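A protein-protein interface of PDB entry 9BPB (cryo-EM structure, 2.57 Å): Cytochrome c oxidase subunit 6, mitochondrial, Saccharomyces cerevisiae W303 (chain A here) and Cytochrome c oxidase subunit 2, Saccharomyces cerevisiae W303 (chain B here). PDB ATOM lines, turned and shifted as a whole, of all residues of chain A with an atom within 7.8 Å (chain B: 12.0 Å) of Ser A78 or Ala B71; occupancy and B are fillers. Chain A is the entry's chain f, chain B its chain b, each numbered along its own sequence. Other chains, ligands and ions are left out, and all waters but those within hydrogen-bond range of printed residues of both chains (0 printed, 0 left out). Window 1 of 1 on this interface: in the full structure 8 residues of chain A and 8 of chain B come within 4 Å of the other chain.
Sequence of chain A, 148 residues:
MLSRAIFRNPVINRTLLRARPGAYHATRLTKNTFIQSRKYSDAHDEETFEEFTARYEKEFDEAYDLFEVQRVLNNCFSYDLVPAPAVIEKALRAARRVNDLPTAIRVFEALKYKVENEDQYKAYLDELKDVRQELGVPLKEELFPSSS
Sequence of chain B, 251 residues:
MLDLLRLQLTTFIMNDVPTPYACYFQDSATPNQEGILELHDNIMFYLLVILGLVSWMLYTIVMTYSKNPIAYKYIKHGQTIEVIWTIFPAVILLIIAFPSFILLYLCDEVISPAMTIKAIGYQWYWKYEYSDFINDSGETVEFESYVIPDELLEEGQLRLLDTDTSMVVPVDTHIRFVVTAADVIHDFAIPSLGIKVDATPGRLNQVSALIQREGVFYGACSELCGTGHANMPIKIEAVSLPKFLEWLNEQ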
ATOM      1  N   PHE A  52      37.738 -26.548 -29.447  1.00  0.00           N
ATOM      2  CA  PHE A  52      36.386 -25.999 -29.476  1.00  0.00           C
ATOM      3  C   PHE A  52      35.422 -26.952 -30.172  1.00  0.00           C
ATOM      4  O   PHE A  52      34.349 -27.267 -29.644  1.00  0.00           O
ATOM      5  CB  PHE A  52      36.414 -24.631 -30.168  1.00  0.00           C
ATOM      6  CG  PHE A  52      35.072 -23.948 -30.269  1.00  0.00           C
ATOM      7  CD1 PHE A  52      34.136 -24.342 -31.212  1.00  0.00           C
ATOM      8  CD2 PHE A  52      34.766 -22.887 -29.437  1.00  0.00           C
ATOM      9  CE1 PHE A  52      32.913 -23.707 -31.305  1.00  0.00           C
ATOM     10  CE2 PHE A  52      33.544 -22.244 -29.530  1.00  0.00           C
ATOM     11  CZ  PHE A  52      32.619 -22.656 -30.466  1.00  0.00           C
ATOM     12  N   TYR A  56      32.106 -29.053 -28.216  1.00  0.00           N
ATOM     13  CA  TYR A  56      30.697 -28.901 -28.557  1.00  0.00           C
ATOM     14  C   TYR A  56      30.151 -30.086 -29.331  1.00  0.00           C
ATOM     15  O   TYR A  56      28.932 -30.276 -29.365  1.00  0.00           O
ATOM     16  CB  TYR A  56      30.461 -27.616 -29.347  1.00  0.00           C
ATOM     17  CG  TYR A  56      30.432 -26.390 -28.477  1.00  0.00           C
ATOM     18  CD1 TYR A  56      30.272 -26.506 -27.108  1.00  0.00           C
ATOM     19  CD2 TYR A  56      30.530 -25.121 -29.020  1.00  0.00           C
ATOM     20  CE1 TYR A  56      30.230 -25.401 -26.300  1.00  0.00           C
ATOM     21  CE2 TYR A  56      30.486 -24.005 -28.217  1.00  0.00           C
ATOM     22  CZ  TYR A  56      30.336 -24.152 -26.856  1.00  0.00           C
ATOM     23  OH  TYR A  56      30.290 -23.051 -26.039  1.00  0.00           O
ATOM     24  N   ARG A  71      19.595 -24.059 -25.566  1.00  0.00           N
ATOM     25  CA  ARG A  71      20.591 -23.410 -24.718  1.00  0.00           C
ATOM     26  C   ARG A  71      21.999 -23.627 -25.258  1.00  0.00           C
ATOM     27  O   ARG A  71      22.835 -22.715 -25.214  1.00  0.00           O
ATOM     28  CB  ARG A  71      20.480 -23.930 -23.287  1.00  0.00           C
ATOM     29  CG  ARG A  71      21.570 -23.422 -22.356  1.00  0.00           C
ATOM     30  CD  ARG A  71      21.550 -24.152 -21.024  1.00  0.00           C
ATOM     31  NE  ARG A  71      22.269 -25.420 -21.079  1.00  0.00           N
ATOM     32  CZ  ARG A  71      23.588 -25.535 -21.135  1.00  0.00           C
ATOM     33  NH1 ARG A  71      24.376 -24.472 -21.131  1.00  0.00           N
ATOM     34  NH2 ARG A  71      24.132 -26.746 -21.198  1.00  0.00           N
ATOM     35  N   VAL A  72      22.284 -24.829 -25.766  1.00  0.00           N
ATOM     36  CA  VAL A  72      23.614 -25.120 -26.289  1.00  0.00           C
ATOM     37  C   VAL A  72      23.858 -24.371 -27.594  1.00  0.00           C
ATOM     38  O   VAL A  72      24.929 -23.786 -27.796  1.00  0.00           O
ATOM     39  CB  VAL A  72      23.802 -26.638 -26.461  1.00  0.00           C
ATOM     40  CG1 VAL A  72      25.138 -26.939 -27.110  1.00  0.00           C
ATOM     41  CG2 VAL A  72      23.700 -27.337 -25.119  1.00  0.00           C
ATOM     42  N   LEU A  73      22.875 -24.369 -28.500  1.00  0.00           N
ATOM     43  CA  LEU A  73      23.058 -23.681 -29.775  1.00  0.00           C
ATOM     44  C   LEU A  73      23.164 -22.172 -29.594  1.00  0.00           C
ATOM     45  O   LEU A  73      23.787 -21.495 -30.415  1.00  0.00           O
ATOM     46  CB  LEU A  73      21.919 -24.025 -30.735  1.00  0.00           C
ATOM     47  CG  LEU A  73      22.183 -23.706 -32.211  1.00  0.00           C
ATOM     48  CD1 LEU A  73      22.999 -24.799 -32.870  1.00  0.00           C
ATOM     49  CD2 LEU A  73      20.885 -23.497 -32.965  1.00  0.00           C
ATOM     50  N   ASN A  74      22.562 -21.626 -28.535  1.00  0.00           N
ATOM     51  CA  ASN A  74      22.760 -20.214 -28.237  1.00  0.00           C
ATOM     52  C   ASN A  74      24.145 -19.963 -27.660  1.00  0.00           C
ATOM     53  O   ASN A  74      24.609 -18.819 -27.645  1.00  0.00           O
ATOM     54  CB  ASN A  74      21.685 -19.719 -27.271  1.00  0.00           C
ATOM     55  CG  ASN A  74      21.630 -18.208 -27.183  1.00  0.00           C
ATOM     56  OD1 ASN A  74      21.211 -17.535 -28.124  1.00  0.00           O
ATOM     57  ND2 ASN A  74      22.055 -17.664 -26.050  1.00  0.00           N
ATOM     58  N   ASN A  75      24.811 -21.013 -27.178  1.00  0.00           N
ATOM     59  CA  ASN A  75      26.184 -20.877 -26.707  1.00  0.00           C
ATOM     60  C   ASN A  75      27.181 -21.067 -27.844  1.00  0.00           C
ATOM     61  O   ASN A  75      28.196 -20.365 -27.904  1.00  0.00           O
ATOM     62  CB  ASN A  75      26.458 -21.881 -25.588  1.00  0.00           C
ATOM     63  CG  ASN A  75      25.847 -21.462 -24.268  1.00  0.00           C
ATOM     64  OD1 ASN A  75      26.105 -20.367 -23.770  1.00  0.00           O
ATOM     65  ND2 ASN A  75      25.030 -22.335 -23.692  1.00  0.00           N
ATOM     66  N   CYS A  76      26.905 -22.007 -28.752  1.00  0.00           N
ATOM     67  CA  CYS A  76      27.819 -22.272 -29.858  1.00  0.00           C
ATOM     68  C   CYS A  76      27.924 -21.080 -30.799  1.00  0.00           C
ATOM     69  O   CYS A  76      29.017 -20.751 -31.273  1.00  0.00           O
ATOM     70  CB  CYS A  76      27.368 -23.514 -30.622  1.00  0.00           C
ATOM     71  SG  CYS A  76      28.617 -24.174 -31.735  1.00  0.00           S
ATOM     72  N   PHE A  77      26.804 -20.427 -31.092  1.00  0.00           N
ATOM     73  CA  PHE A  77      26.812 -19.265 -31.972  1.00  0.00           C
ATOM     74  C   PHE A  77      27.086 -17.967 -31.232  1.00  0.00           C
ATOM     75  O   PHE A  77      27.109 -16.907 -31.865  1.00  0.00           O
ATOM     76  CB  PHE A  77      25.484 -19.166 -32.726  1.00  0.00           C
ATOM     77  CG  PHE A  77      25.441 -19.992 -33.977  1.00  0.00           C
ATOM     78  CD1 PHE A  77      26.074 -19.558 -35.129  1.00  0.00           C
ATOM     79  CD2 PHE A  77      24.782 -21.207 -34.002  1.00  0.00           C
ATOM     80  CE1 PHE A  77      26.043 -20.316 -36.279  1.00  0.00           C
ATOM     81  CE2 PHE A  77      24.749 -21.971 -35.150  1.00  0.00           C
ATOM     82  CZ  PHE A  77      25.380 -21.525 -36.290  1.00  0.00           C
ATOM     83  N   SER A  78      27.290 -18.020 -29.916  1.00  0.00           N
ATOM     84  CA  SER A  78      27.627 -16.818 -29.169  1.00  0.00           C
ATOM     85  C   SER A  78      29.126 -16.552 -29.165  1.00  0.00           C
ATOM     86  O   SER A  78      29.556 -15.484 -28.719  1.00  0.00           O
ATOM     87  CB  SER A  78      27.109 -16.928 -27.736  1.00  0.00           C
ATOM     88  OG  SER A  78      27.717 -18.015 -27.062  1.00  0.00           O
ATOM     89  N   TYR A  79      29.927 -17.497 -29.650  1.00  0.00           N
ATOM     90  CA  TYR A  79      31.366 -17.298 -29.693  1.00  0.00           C
ATOM     91  C   TYR A  79      31.765 -16.543 -30.954  1.00  0.00           C
ATOM     92  O   TYR A  79      31.048 -16.539 -31.957  1.00  0.00           O
ATOM     93  CB  TYR A  79      32.102 -18.636 -29.628  1.00  0.00           C
ATOM     94  CG  TYR A  79      32.229 -19.187 -28.228  1.00  0.00           C
ATOM     95  CD1 TYR A  79      31.141 -19.748 -27.582  1.00  0.00           C
ATOM     96  CD2 TYR A  79      33.437 -19.134 -27.550  1.00  0.00           C
ATOM     97  CE1 TYR A  79      31.248 -20.249 -26.304  1.00  0.00           C
ATOM     98  CE2 TYR A  79      33.557 -19.634 -26.268  1.00  0.00           C
ATOM     99  CZ  TYR A  79      32.458 -20.191 -25.651  1.00  0.00           C
ATOM    100  OH  TYR A  79      32.570 -20.691 -24.375  1.00  0.00           O
ATOM    101  N   ASP A  80      32.932 -15.898 -30.888  1.00  0.00           N
ATOM    102  CA  ASP A  80      33.378 -15.039 -31.982  1.00  0.00           C
ATOM    103  C   ASP A  80      33.604 -15.839 -33.260  1.00  0.00           C
ATOM    104  O   ASP A  80      33.260 -15.385 -34.358  1.00  0.00           O
ATOM    105  CB  ASP A  80      34.652 -14.306 -31.566  1.00  0.00           C
ATOM    106  CG  ASP A  80      35.042 -13.211 -32.535  1.00  0.00           C
ATOM    107  OD1 ASP A  80      34.279 -12.953 -33.489  1.00  0.00           O
ATOM    108  OD2 ASP A  80      36.110 -12.599 -32.331  1.00  0.00           O
ATOM    109  N   LEU A  81      34.180 -17.028 -33.136  1.00  0.00           N
ATOM    110  CA  LEU A  81      34.442 -17.868 -34.295  1.00  0.00           C
ATOM    111  C   LEU A  81      33.142 -18.397 -34.894  1.00  0.00           C
ATOM    112  O   LEU A  81      32.183 -18.699 -34.178  1.00  0.00           O
ATOM    113  CB  LEU A  81      35.366 -19.018 -33.888  1.00  0.00           C
ATOM    114  CG  LEU A  81      34.912 -20.028 -32.820  1.00  0.00           C
ATOM    115  CD1 LEU A  81      34.041 -21.130 -33.404  1.00  0.00           C
ATOM    116  CD2 LEU A  81      36.098 -20.620 -32.069  1.00  0.00           C
ATOM    117  N   PRO A  83      31.293 -21.498 -36.275  1.00  0.00           N
ATOM    118  CA  PRO A  83      31.551 -22.919 -36.022  1.00  0.00           C
ATOM    119  C   PRO A  83      31.891 -23.679 -37.296  1.00  0.00           C
ATOM    120  O   PRO A  83      31.504 -23.295 -38.402  1.00  0.00           O
ATOM    121  CB  PRO A  83      30.234 -23.415 -35.412  1.00  0.00           C
ATOM    122  CG  PRO A  83      29.213 -22.403 -35.830  1.00  0.00           C
ATOM    123  CD  PRO A  83      29.943 -21.102 -35.847  1.00  0.00           C
ATOM    124  N   LYS A 114      25.771 -15.407 -39.402  1.00  0.00           N
ATOM    125  CA  LYS A 114      27.052 -15.635 -38.743  1.00  0.00           C
ATOM    126  C   LYS A 114      28.196 -15.832 -39.729  1.00  0.00           C
ATOM    127  O   LYS A 114      29.310 -15.365 -39.472  1.00  0.00           O
ATOM    128  CB  LYS A 114      26.958 -16.853 -37.824  1.00  0.00           C
ATOM    129  CG  LYS A 114      28.172 -17.067 -36.944  1.00  0.00           C
ATOM    130  CD  LYS A 114      28.326 -15.965 -35.918  1.00  0.00           C
ATOM    131  CE  LYS A 114      29.387 -16.329 -34.899  1.00  0.00           C
ATOM    132  NZ  LYS A 114      29.423 -15.364 -33.777  1.00  0.00           N
ATOM    133  N   ILE B  61      28.760   1.675 -33.237  1.00  0.00           N
ATOM    134  CA  ILE B  61      28.187   0.625 -32.399  1.00  0.00           C
ATOM    135  C   ILE B  61      26.666   0.715 -32.397  1.00  0.00           C
ATOM    136  O   ILE B  61      25.968  -0.304 -32.485  1.00  0.00           O
ATOM    137  CB  ILE B  61      28.762   0.715 -30.973  1.00  0.00           C
ATOM    138  CG1 ILE B  61      30.221   0.257 -30.957  1.00  0.00           C
ATOM    139  CG2 ILE B  61      27.938  -0.115 -30.011  1.00  0.00           C
ATOM    140  CD1 ILE B  61      30.931   0.523 -29.650  1.00  0.00           C
ATOM    141  N   THR B  64      25.457  -0.387 -36.021  1.00  0.00           N
ATOM    142  CA  THR B  64      25.806  -1.722 -36.501  1.00  0.00           C
ATOM    143  C   THR B  64      25.184  -2.816 -35.643  1.00  0.00           C
ATOM    144  O   THR B  64      24.653  -3.798 -36.172  1.00  0.00           O
ATOM    145  CB  THR B  64      27.324  -1.888 -36.546  1.00  0.00           C
ATOM    146  OG1 THR B  64      27.908  -0.758 -37.203  1.00  0.00           O
ATOM    147  CG2 THR B  64      27.702  -3.160 -37.286  1.00  0.00           C
ATOM    148  N   TYR B  65      25.239  -2.671 -34.321  1.00  0.00           N
ATOM    149  CA  TYR B  65      24.848  -3.745 -33.422  1.00  0.00           C
ATOM    150  C   TYR B  65      23.439  -3.609 -32.867  1.00  0.00           C
ATOM    151  O   TYR B  65      22.966  -4.537 -32.204  1.00  0.00           O
ATOM    152  CB  TYR B  65      25.859  -3.861 -32.274  1.00  0.00           C
ATOM    153  CG  TYR B  65      27.199  -4.376 -32.747  1.00  0.00           C
ATOM    154  CD1 TYR B  65      27.436  -5.740 -32.855  1.00  0.00           C
ATOM    155  CD2 TYR B  65      28.211  -3.502 -33.123  1.00  0.00           C
ATOM    156  CE1 TYR B  65      28.650  -6.219 -33.296  1.00  0.00           C
ATOM    157  CE2 TYR B  65      29.433  -3.974 -33.568  1.00  0.00           C
ATOM    158  CZ  TYR B  65      29.643  -5.335 -33.652  1.00  0.00           C
ATOM    159  OH  TYR B  65      30.854  -5.817 -34.092  1.00  0.00           O
ATOM    160  N   SER B  66      22.757  -2.489 -33.111  1.00  0.00           N
ATOM    161  CA  SER B  66      21.310  -2.480 -32.936  1.00  0.00           C
ATOM    162  C   SER B  66      20.653  -3.454 -33.897  1.00  0.00           C
ATOM    163  O   SER B  66      19.602  -4.026 -33.585  1.00  0.00           O
ATOM    164  CB  SER B  66      20.753  -1.074 -33.138  1.00  0.00           C
ATOM    165  OG  SER B  66      19.361  -1.111 -33.383  1.00  0.00           O
ATOM    166  N   LYS B  67      21.262  -3.656 -35.065  1.00  0.00           N
ATOM    167  CA  LYS B  67      20.811  -4.627 -36.051  1.00  0.00           C
ATOM    168  C   LYS B  67      21.543  -5.955 -35.925  1.00  0.00           C
ATOM    169  O   LYS B  67      21.605  -6.719 -36.894  1.00  0.00           O
ATOM    170  CB  LYS B  67      20.988  -4.063 -37.461  1.00  0.00           C
ATOM    171  CG  LYS B  67      20.235  -2.773 -37.721  1.00  0.00           C
ATOM    172  CD  LYS B  67      20.302  -2.394 -39.190  1.00  0.00           C
ATOM    173  CE  LYS B  67      21.710  -1.990 -39.589  1.00  0.00           C
ATOM    174  NZ  LYS B  67      21.789  -1.569 -41.015  1.00  0.00           N
ATOM    175  N   ASN B  68      22.107  -6.241 -34.755  1.00  0.00           N
ATOM    176  CA  ASN B  68      22.842  -7.478 -34.526  1.00  0.00           C
ATOM    177  C   ASN B  68      22.078  -8.346 -33.541  1.00  0.00           C
ATOM    178  O   ASN B  68      22.062  -8.039 -32.340  1.00  0.00           O
ATOM    179  CB  ASN B  68      24.245  -7.183 -33.996  1.00  0.00           C
ATOM    180  CG  ASN B  68      24.988  -8.435 -33.580  1.00  0.00           C
ATOM    181  OD1 ASN B  68      25.198  -9.342 -34.385  1.00  0.00           O
ATOM    182  ND2 ASN B  68      25.393  -8.489 -32.319  1.00  0.00           N
ATOM    183  N   PRO B  69      21.428  -9.412 -33.983  1.00  0.00           N
ATOM    184  CA  PRO B  69      20.702 -10.269 -33.040  1.00  0.00           C
ATOM    185  C   PRO B  69      21.613 -10.954 -32.034  1.00  0.00           C
ATOM    186  O   PRO B  69      21.404 -10.838 -30.824  1.00  0.00           O
ATOM    187  CB  PRO B  69      20.007 -11.285 -33.954  1.00  0.00           C
ATOM    188  CG  PRO B  69      20.806 -11.288 -35.207  1.00  0.00           C
ATOM    189  CD  PRO B  69      21.320  -9.892 -35.369  1.00  0.00           C
ATOM    190  N   ILE B  70      22.635 -11.659 -32.519  1.00  0.00           N
ATOM    191  CA  ILE B  70      23.462 -12.481 -31.643  1.00  0.00           C
ATOM    192  C   ILE B  70      24.388 -11.594 -30.825  1.00  0.00           C
ATOM    193  O   ILE B  70      25.017 -10.668 -31.350  1.00  0.00           O
ATOM    194  CB  ILE B  70      24.249 -13.513 -32.463  1.00  0.00           C
ATOM    195  CG1 ILE B  70      23.288 -14.521 -33.096  1.00  0.00           C
ATOM    196  CG2 ILE B  70      25.267 -14.224 -31.590  1.00  0.00           C
ATOM    197  CD1 ILE B  70      23.921 -15.392 -34.151  1.00  0.00           C
ATOM    198  N   ALA B  71      24.475 -11.877 -29.526  1.00  0.00           N
ATOM    199  CA  ALA B  71      25.311 -11.130 -28.601  1.00  0.00           C
ATOM    200  C   ALA B  71      26.423 -12.029 -28.081  1.00  0.00           C
ATOM    201  O   ALA B  71      26.158 -13.119 -27.564  1.00  0.00           O
ATOM    202  CB  ALA B  71      24.484 -10.587 -27.434  1.00  0.00           C
ATOM    203  N   TYR B  72      27.664 -11.564 -28.208  1.00  0.00           N
ATOM    204  CA  TYR B  72      28.839 -12.330 -27.794  1.00  0.00           C
ATOM    205  C   TYR B  72      29.033 -12.097 -26.303  1.00  0.00           C
ATOM    206  O   TYR B  72      29.786 -11.219 -25.884  1.00  0.00           O
ATOM    207  CB  TYR B  72      30.070 -11.916 -28.592  1.00  0.00           C
ATOM    208  CG  TYR B  72      29.959 -12.114 -30.091  1.00  0.00           C
ATOM    209  CD1 TYR B  72      28.848 -12.728 -30.656  1.00  0.00           C
ATOM    210  CD2 TYR B  72      30.963 -11.678 -30.942  1.00  0.00           C
ATOM    211  CE1 TYR B  72      28.742 -12.898 -32.017  1.00  0.00           C
ATOM    212  CE2 TYR B  72      30.867 -11.849 -32.304  1.00  0.00           C
ATOM    213  CZ  TYR B  72      29.755 -12.460 -32.837  1.00  0.00           C
ATOM    214  OH  TYR B  72      29.652 -12.637 -34.196  1.00  0.00           O
ATOM    215  N   LYS B  73      28.373 -12.920 -25.486  1.00  0.00           N
ATOM    216  CA  LYS B  73      28.264 -12.673 -24.054  1.00  0.00           C
ATOM    217  C   LYS B  73      29.413 -13.280 -23.257  1.00  0.00           C
ATOM    218  O   LYS B  73      29.225 -13.647 -22.090  1.00  0.00           O
ATOM    219  CB  LYS B  73      26.924 -13.190 -23.527  1.00  0.00           C
ATOM    220  CG  LYS B  73      26.652 -14.657 -23.793  1.00  0.00           C
ATOM    221  CD  LYS B  73      25.257 -15.043 -23.333  1.00  0.00           C
ATOM    222  CE  LYS B  73      24.935 -16.482 -23.688  1.00  0.00           C
ATOM    223  NZ  LYS B  73      25.738 -17.451 -22.897  1.00  0.00           N
ATOM    224  N   TYR B  74      30.600 -13.408 -23.854  1.00  0.00           N
ATOM    225  CA  TYR B  74      31.744 -13.988 -23.163  1.00  0.00           C
ATOM    226  C   TYR B  74      33.005 -13.149 -23.349  1.00  0.00           C
ATOM    227  O   TYR B  74      34.118 -13.661 -23.210  1.00  0.00           O
ATOM    228  CB  TYR B  74      31.992 -15.419 -23.637  1.00  0.00           C
ATOM    229  CG  TYR B  74      30.871 -16.379 -23.321  1.00  0.00           C
ATOM    230  CD1 TYR B  74      30.404 -16.531 -22.023  1.00  0.00           C
ATOM    231  CD2 TYR B  74      30.288 -17.145 -24.320  1.00  0.00           C
ATOM    232  CE1 TYR B  74      29.383 -17.412 -21.733  1.00  0.00           C
ATOM    233  CE2 TYR B  74      29.267 -18.028 -24.039  1.00  0.00           C
ATOM    234  CZ  TYR B  74      28.818 -18.157 -22.744  1.00  0.00           C
ATOM    235  OH  TYR B  74      27.801 -19.036 -22.459  1.00  0.00           O
ATOM    236  N   ILE B  75      32.856 -11.866 -23.652  1.00  0.00           N
ATOM    237  CA  ILE B  75      33.995 -10.972 -23.874  1.00  0.00           C
ATOM    238  C   ILE B  75      34.032 -10.005 -22.698  1.00  0.00           C
ATOM    239  O   ILE B  75      33.342  -8.980 -22.680  1.00  0.00           O
ATOM    240  CB  ILE B  75      33.908 -10.234 -25.211  1.00  0.00           C
ATOM    241  CG1 ILE B  75      33.944 -11.232 -26.369  1.00  0.00           C
ATOM    242  CG2 ILE B  75      35.043  -9.233 -25.346  1.00  0.00           C
ATOM    243  CD1 ILE B  75      33.964 -10.583 -27.729  1.00  0.00           C
ATOM    244  N   LYS B  76      34.849 -10.327 -21.694  1.00  0.00           N
ATOM    245  CA  LYS B  76      34.895  -9.535 -20.471  1.00  0.00           C
ATOM    246  C   LYS B  76      36.315  -9.133 -20.088  1.00  0.00           C
ATOM    247  O   LYS B  76      36.524  -8.050 -19.534  1.00  0.00           O
ATOM    248  CB  LYS B  76      34.242 -10.304 -19.319  1.00  0.00           C
ATOM    249  CG  LYS B  76      32.847 -10.810 -19.631  1.00  0.00           C
ATOM    250  CD  LYS B  76      32.233 -11.545 -18.453  1.00  0.00           C
ATOM    251  CE  LYS B  76      32.634 -13.008 -18.439  1.00  0.00           C
ATOM    252  NZ  LYS B  76      31.729 -13.816 -17.576  1.00  0.00           N
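Arg A71 touches none of the printed residues of chain B. Asn A74 touches just one residue of chain B: Lys B73 (3.9 Å). Of chain B, only Lys B73 and Tyr B74 come within 4 Å of Asn A75. No residue of chain B comes within 4 Å of Cys A76. Printed residues of chain B within 4 Å of Phe A77: Ile B70 (3.3 Å). Of chain B, only Ala B71, Tyr B72 and Tyr B74 come within 4 Å of Ser A78. Tyr A79 touches just one residue of chain B: Tyr B74. Printed residues of chain B within 4 Å of Asp A80: Tyr B72 (3.8 Å). Of the printed residues of chain B, Lys A114 touches Tyr B72 (2.8 Å). Of the printed residues of chain A, Tyr B72 touches Ser A78 (3.4 Å), Asp A80 (3.8 Å) and Lys A114 (2.8 Å). Printed residues of chain A within 4 Å of Lys B73: Asn A74 and Asn A75. Of the printed residues of chain A, Tyr B74 touches Asn A75 (2.5 Å), Ser A78 (3.4 Å) and Tyr A79 (3.7 Å). The nearest residue of chain B that does not touch Ser A78 is Ile B70 (4.3 Å). The nearest residue of chain A that does not touch Ala B71 is Phe A77 (5.8 Å).
NZ of Lys B73 sits at hydrogen-bond distance from OD1 of Asn A75. The side-chain amino group of Lys A114 sits at hydrogen-bond distance from the side-chain hydroxyl of Tyr B72. The side-chain hydroxyl (OH) of Tyr B74 is in hydrogen-bond range of the side-chain amide oxygen (OD1) of Asn A75 (2.5 Å).
The backbone carbonyl oxygen (O) of Phe A77 lies within hydrogen-bond range of the side-chain amino group (NZ) of Lys A114 (3.4 Å). The backbone carbonyl oxygen (O) of Arg A71 is in hydrogen-bond range of the side-chain amide nitrogen (ND2) of Asn A75 (2.7 Å). The backbone carbonyl oxygen of Tyr A79 is in hydrogen-bond range of the side-chain amino group of Lys A114. The side-chain hydroxyl (OG) of Ser A78 lies within hydrogen-bond range of the backbone carbonyl oxygen (O) of Asn A75, at 2.5 Å. The side-chain amino group (NZ) of Lys B73 sits at hydrogen-bond distance from the side-chain hydroxyl (OH) of Tyr B74, at 2.6 Å. The backbone carbonyl oxygen (O) of Asn A74 sits close to the side-chain hydroxyl (OG) of Ser A78.
Of the 15 printed residues of chain A, 7 touch a printed residue of chain B. Hydrophobic or aromatic side chains of chain A within 4 Å of the printed part of chain B: Tyr A79. Of the 14 printed residues of chain B, 5 touch a printed residue of chain A. Among the printed residues, 10 pairs touch across the chains. Among the printed residues, no Asp or Glu carboxylate lies within 4 Å of a Lys or Arg side-chain nitrogen of the other chain.
Among the printed residues, pairs that only touch across the chains: Phe A77 with Ile B70, Ser A78 with Tyr B72, Ser A78 with Tyr B74, Tyr A79 with Tyr B74, Asp A80 with Tyr B72, Asn A74 with Lys B73 and Ser A78 with Ala B71.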
